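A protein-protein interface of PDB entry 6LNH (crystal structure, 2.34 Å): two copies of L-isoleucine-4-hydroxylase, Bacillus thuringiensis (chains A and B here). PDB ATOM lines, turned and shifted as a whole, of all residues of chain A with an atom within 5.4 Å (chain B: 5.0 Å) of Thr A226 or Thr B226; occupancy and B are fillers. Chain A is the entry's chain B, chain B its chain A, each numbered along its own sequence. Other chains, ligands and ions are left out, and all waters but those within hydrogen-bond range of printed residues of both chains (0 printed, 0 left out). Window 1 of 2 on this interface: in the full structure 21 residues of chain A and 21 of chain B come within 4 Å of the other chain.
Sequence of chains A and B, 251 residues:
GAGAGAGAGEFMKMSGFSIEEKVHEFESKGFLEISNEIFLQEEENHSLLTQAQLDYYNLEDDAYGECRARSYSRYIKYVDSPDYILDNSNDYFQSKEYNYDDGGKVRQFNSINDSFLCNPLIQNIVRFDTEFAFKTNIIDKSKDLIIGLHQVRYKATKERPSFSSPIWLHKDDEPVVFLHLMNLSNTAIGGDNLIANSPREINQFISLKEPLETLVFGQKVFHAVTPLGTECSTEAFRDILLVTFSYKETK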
ATOM      1  N   SER A 162      24.068 -22.435   8.287  1.00  0.00           N
ATOM      2  CA  SER A 162      24.689 -23.384   7.327  1.00  0.00           C
ATOM      3  C   SER A 162      23.651 -24.362   6.767  1.00  0.00           C
ATOM      4  O   SER A 162      22.872 -24.907   7.562  1.00  0.00           O
ATOM      5  CB  SER A 162      25.824 -24.119   7.982  1.00  0.00           C
ATOM      6  OG  SER A 162      26.282 -25.173   7.158  1.00  0.00           O
ATOM      7  N   GLY A 190      19.993 -26.908  15.663  1.00  0.00           N
ATOM      8  CA  GLY A 190      19.710 -27.607  14.435  1.00  0.00           C
ATOM      9  C   GLY A 190      20.694 -28.730  14.171  1.00  0.00           C
ATOM     10  O   GLY A 190      21.332 -29.285  15.073  1.00  0.00           O
ATOM     11  N   GLY A 191      20.815 -29.063  12.890  1.00  0.00           N
ATOM     12  CA  GLY A 191      21.624 -30.198  12.497  1.00  0.00           C
ATOM     13  C   GLY A 191      21.009 -31.519  12.888  1.00  0.00           C
ATOM     14  O   GLY A 191      21.731 -32.499  13.092  1.00  0.00           O
ATOM     15  N   ASP A 192      19.685 -31.569  12.999  1.00  0.00           N
ATOM     16  CA  ASP A 192      18.991 -32.808  13.305  1.00  0.00           C
ATOM     17  C   ASP A 192      18.758 -33.612  12.033  1.00  0.00           C
ATOM     18  O   ASP A 192      18.567 -33.058  10.947  1.00  0.00           O
ATOM     19  CB  ASP A 192      17.664 -32.509  13.999  1.00  0.00           C
ATOM     20  CG  ASP A 192      17.825 -31.565  15.178  1.00  0.00           C
ATOM     21  OD1 ASP A 192      18.764 -31.765  15.978  1.00  0.00           O
ATOM     22  OD2 ASP A 192      17.016 -30.620  15.301  1.00  0.00           O
ATOM     23  N   ASN A 193      18.765 -34.934  12.179  1.00  0.00           N
ATOM     24  CA  ASN A 193      18.622 -35.843  11.050  1.00  0.00           C
ATOM     25  C   ASN A 193      17.181 -36.325  10.943  1.00  0.00           C
ATOM     26  O   ASN A 193      16.565 -36.694  11.949  1.00  0.00           O
ATOM     27  CB  ASN A 193      19.578 -37.026  11.191  1.00  0.00           C
ATOM     28  CG  ASN A 193      21.022 -36.631  10.953  1.00  0.00           C
ATOM     29  OD1 ASN A 193      21.832 -36.612  11.879  1.00  0.00           O
ATOM     30  ND2 ASN A 193      21.348 -36.300   9.709  1.00  0.00           N
ATOM     31  N   LEU A 194      16.654 -36.313   9.724  1.00  0.00           N
ATOM     32  CA  LEU A 194      15.285 -36.719   9.443  1.00  0.00           C
ATOM     33  C   LEU A 194      15.280 -37.957   8.559  1.00  0.00           C
ATOM     34  O   LEU A 194      16.122 -38.101   7.671  1.00  0.00           O
ATOM     35  CB  LEU A 194      14.512 -35.583   8.767  1.00  0.00           C
ATOM     36  CG  LEU A 194      14.611 -34.252   9.512  1.00  0.00           C
ATOM     37  CD1 LEU A 194      13.941 -33.139   8.726  1.00  0.00           C
ATOM     38  CD2 LEU A 194      14.001 -34.383  10.901  1.00  0.00           C
ATOM     39  N   ALA A 224      17.532 -36.303   5.555  1.00  0.00           N
ATOM     40  CA  ALA A 224      17.890 -34.897   5.466  1.00  0.00           C
ATOM     41  C   ALA A 224      18.604 -34.492   6.744  1.00  0.00           C
ATOM     42  O   ALA A 224      18.574 -35.205   7.751  1.00  0.00           O
ATOM     43  CB  ALA A 224      16.654 -34.020   5.231  1.00  0.00           C
ATOM     44  N   VAL A 225      19.256 -33.335   6.689  1.00  0.00           N
ATOM     45  CA  VAL A 225      19.837 -32.704   7.865  1.00  0.00           C
ATOM     46  C   VAL A 225      19.246 -31.304   7.986  1.00  0.00           C
ATOM     47  O   VAL A 225      19.252 -30.530   7.020  1.00  0.00           O
ATOM     48  CB  VAL A 225      21.377 -32.682   7.809  1.00  0.00           C
ATOM     49  CG1 VAL A 225      21.896 -31.799   6.675  1.00  0.00           C
ATOM     50  CG2 VAL A 225      21.951 -32.244   9.149  1.00  0.00           C
ATOM     51  N   THR A 226      18.655 -31.020   9.143  1.00  0.00           N
ATOM     52  CA  THR A 226      18.112 -29.701   9.413  1.00  0.00           C
ATOM     53  C   THR A 226      19.241 -28.666   9.374  1.00  0.00           C
ATOM     54  O   THR A 226      20.388 -28.980   9.709  1.00  0.00           O
ATOM     55  CB  THR A 226      17.402 -29.729  10.773  1.00  0.00           C
ATOM     56  OG1 THR A 226      16.083 -30.276  10.618  1.00  0.00           O
ATOM     57  CG2 THR A 226      17.323 -28.359  11.435  1.00  0.00           C
ATOM     58  N   PRO A 227      18.958 -27.433   8.939  1.00  0.00           N
ATOM     59  CA  PRO A 227      20.004 -26.403   8.927  1.00  0.00           C
ATOM     60  C   PRO A 227      20.597 -26.169  10.309  1.00  0.00           C
ATOM     61  O   PRO A 227      19.967 -26.433  11.335  1.00  0.00           O
ATOM     62  CB  PRO A 227      19.271 -25.158   8.414  1.00  0.00           C
ATOM     63  CG  PRO A 227      18.147 -25.713   7.607  1.00  0.00           C
ATOM     64  CD  PRO A 227      17.703 -26.936   8.351  1.00  0.00           C
ATOM     65  N   LEU A 228      21.831 -25.672  10.322  1.00  0.00           N
ATOM     66  CA  LEU A 228      22.546 -25.345  11.550  1.00  0.00           C
ATOM     67  C   LEU A 228      22.516 -23.838  11.769  1.00  0.00           C
ATOM     68  O   LEU A 228      22.859 -23.068  10.864  1.00  0.00           O
ATOM     69  CB  LEU A 228      23.993 -25.841  11.482  1.00  0.00           C
ATOM     70  CG  LEU A 228      24.827 -25.835  12.764  1.00  0.00           C
ATOM     71  CD1 LEU A 228      24.487 -27.029  13.643  1.00  0.00           C
ATOM     72  CD2 LEU A 228      26.313 -25.821  12.427  1.00  0.00           C
ATOM     73  N   GLY B 190      13.847 -29.618  17.992  1.00  0.00           N
ATOM     74  CA  GLY B 190      13.369 -29.181  16.703  1.00  0.00           C
ATOM     75  C   GLY B 190      12.341 -28.078  16.863  1.00  0.00           C
ATOM     76  O   GLY B 190      12.301 -27.362  17.867  1.00  0.00           O
ATOM     77  N   GLY B 191      11.498 -27.939  15.845  1.00  0.00           N
ATOM     78  CA  GLY B 191      10.546 -26.847  15.846  1.00  0.00           C
ATOM     79  C   GLY B 191      11.194 -25.498  15.654  1.00  0.00           C
ATOM     80  O   GLY B 191      10.669 -24.487  16.128  1.00  0.00           O
ATOM     81  N   ASP B 192      12.337 -25.461  14.979  1.00  0.00           N
ATOM     82  CA  ASP B 192      13.014 -24.213  14.675  1.00  0.00           C
ATOM     83  C   ASP B 192      12.437 -23.582  13.412  1.00  0.00           C
ATOM     84  O   ASP B 192      11.988 -24.276  12.496  1.00  0.00           O
ATOM     85  CB  ASP B 192      14.509 -24.456  14.497  1.00  0.00           C
ATOM     86  CG  ASP B 192      15.115 -25.257  15.637  1.00  0.00           C
ATOM     87  OD1 ASP B 192      14.940 -24.857  16.808  1.00  0.00           O
ATOM     88  OD2 ASP B 192      15.770 -26.283  15.362  1.00  0.00           O
ATOM     89  N   LEU B 194      12.701 -21.228   9.996  1.00  0.00           N
ATOM     90  CA  LEU B 194      13.626 -20.888   8.925  1.00  0.00           C
ATOM     91  C   LEU B 194      13.068 -19.742   8.090  1.00  0.00           C
ATOM     92  O   LEU B 194      11.861 -19.675   7.842  1.00  0.00           O
ATOM     93  CB  LEU B 194      13.885 -22.104   8.031  1.00  0.00           C
ATOM     94  CG  LEU B 194      14.215 -23.399   8.776  1.00  0.00           C
ATOM     95  CD1 LEU B 194      14.228 -24.579   7.822  1.00  0.00           C
ATOM     96  CD2 LEU B 194      15.549 -23.274   9.494  1.00  0.00           C
ATOM     97  N   PHE B 205      17.764 -18.208  10.850  1.00  0.00           N
ATOM     98  CA  PHE B 205      17.371 -19.362  11.644  1.00  0.00           C
ATOM     99  C   PHE B 205      16.985 -18.829  13.017  1.00  0.00           C
ATOM    100  O   PHE B 205      17.833 -18.310  13.751  1.00  0.00           O
ATOM    101  CB  PHE B 205      18.537 -20.355  11.711  1.00  0.00           C
ATOM    102  CG  PHE B 205      18.216 -21.679  12.353  1.00  0.00           C
ATOM    103  CD1 PHE B 205      17.754 -21.761  13.656  1.00  0.00           C
ATOM    104  CD2 PHE B 205      18.431 -22.856  11.655  1.00  0.00           C
ATOM    105  CE1 PHE B 205      17.491 -22.985  14.239  1.00  0.00           C
ATOM    106  CE2 PHE B 205      18.165 -24.086  12.232  1.00  0.00           C
ATOM    107  CZ  PHE B 205      17.697 -24.151  13.525  1.00  0.00           C
ATOM    108  N   ALA B 224       9.583 -21.849   7.081  1.00  0.00           N
ATOM    109  CA  ALA B 224       9.260 -23.221   7.444  1.00  0.00           C
ATOM    110  C   ALA B 224       9.533 -23.380   8.932  1.00  0.00           C
ATOM    111  O   ALA B 224      10.201 -22.549   9.553  1.00  0.00           O
ATOM    112  CB  ALA B 224      10.066 -24.230   6.619  1.00  0.00           C
ATOM    113  N   VAL B 225       8.988 -24.448   9.507  1.00  0.00           N
ATOM    114  CA  VAL B 225       9.343 -24.874  10.855  1.00  0.00           C
ATOM    115  C   VAL B 225       9.802 -26.323  10.765  1.00  0.00           C
ATOM    116  O   VAL B 225       9.070 -27.185  10.262  1.00  0.00           O
ATOM    117  CB  VAL B 225       8.188 -24.698  11.857  1.00  0.00           C
ATOM    118  CG1 VAL B 225       6.893 -25.290  11.325  1.00  0.00           C
ATOM    119  CG2 VAL B 225       8.551 -25.302  13.210  1.00  0.00           C
ATOM    120  N   THR B 226      11.024 -26.580  11.220  1.00  0.00           N
ATOM    121  CA  THR B 226      11.585 -27.921  11.222  1.00  0.00           C
ATOM    122  C   THR B 226      10.734 -28.866  12.073  1.00  0.00           C
ATOM    123  O   THR B 226      10.044 -28.427  12.999  1.00  0.00           O
ATOM    124  CB  THR B 226      13.020 -27.883  11.743  1.00  0.00           C
ATOM    125  OG1 THR B 226      13.008 -27.623  13.152  1.00  0.00           O
ATOM    126  CG2 THR B 226      13.800 -26.787  11.038  1.00  0.00           C
ATOM    127  N   PRO B 227      10.742 -30.166  11.761  1.00  0.00           N
ATOM    128  CA  PRO B 227       9.956 -31.122  12.551  1.00  0.00           C
ATOM    129  C   PRO B 227      10.302 -31.091  14.034  1.00  0.00           C
ATOM    130  O   PRO B 227      11.390 -30.684  14.446  1.00  0.00           O
ATOM    131  CB  PRO B 227      10.322 -32.477  11.930  1.00  0.00           C
ATOM    132  CG  PRO B 227      10.736 -32.144  10.534  1.00  0.00           C
ATOM    133  CD  PRO B 227      11.449 -30.826  10.648  1.00  0.00           C
ATOM    134  N   LEU B 228       9.339 -31.531  14.842  1.00  0.00           N
ATOM    135  CA  LEU B 228       9.475 -31.623  16.291  1.00  0.00           C
ATOM    136  C   LEU B 228       9.736 -33.070  16.698  1.00  0.00           C
ATOM    137  O   LEU B 228       9.028 -33.979  16.257  1.00  0.00           O
ATOM    138  CB  LEU B 228       8.215 -31.102  16.984  1.00  0.00           C
ATOM    139  CG  LEU B 228       8.322 -30.826  18.482  1.00  0.00           C
ATOM    140  CD1 LEU B 228       9.103 -29.546  18.737  1.00  0.00           C
ATOM    141  CD2 LEU B 228       6.939 -30.759  19.117  1.00  0.00           C
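The backbone NH (N) of Gly B191 sits at hydrogen-bond distance from the side-chain hydroxyl (OG1) of Thr B226, 3.1 Å away. N of Thr B226 is in hydrogen-bond range of O of Asp B192. N of Gly A191 sits at hydrogen-bond distance from O of Thr A226 (3.2 Å). The backbone NH (N) of Gly A191 is in hydrogen-bond range of the backbone carbonyl oxygen (O) of Pro A227, 3.2 Å away. The backbone carbonyl oxygen of Asp A192 sits at hydrogen-bond distance from the backbone NH of Thr A226 (2.7 Å). The backbone NH of Leu A194 lies within hydrogen-bond range of the backbone carbonyl oxygen of Ala A224 (3.0 Å).
Among the printed residues, merely in contact across the chains: Leu A194 with Pro B227 (3.8 Å), Thr A226 with Thr B226 (3.9 Å) and Pro A227 with Phe B205 (3.1 Å).
Gly A191 touches none of the printed residues of chain B. Printed residues of chain B within 4 Å of Pro A227: Phe B205 (3.1 Å). Printed residues of chain A within 4 Å of Phe B205: Pro A227 (3.1 Å). Thr B226 touches one residue of chain A. Of the printed residues of chain A, Pro B227 touches Leu A194 (3.8 Å). The nearest residue of chain B that does not touch Thr A226 is Phe B205 (4.4 Å). The nearest residue of chain A that does not touch Thr B226 is Pro A227 (4.7 Å). The nearest printed residue of chain A that does not touch Phe B205 is Gly A190 (4.1 Å).
Of the 10 printed residues of chain B, 3 touch a printed residue of chain A. Hydrophobic or aromatic side chains of chain B within 4 Å of the printed part of chain A: Phe B205 and Pro B227. Among the printed residues, 3 pairs touch across the chains. Among the printed residues, no Asp or Glu carboxylate lies within 4 Å of a Lys or Arg side-chain nitrogen of the other chain.
Leu A194 touches Pro B227, but with the chains exchanged Pro A227 does not touch Leu B194 (4.03 Å). Thr A226 touches its own counterpart, Thr B226. 9 positions are printed for both chains. Of the 3 pairs that touch across the chains among the printed residues, 1 has its exchanged pair printed and touching as well.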
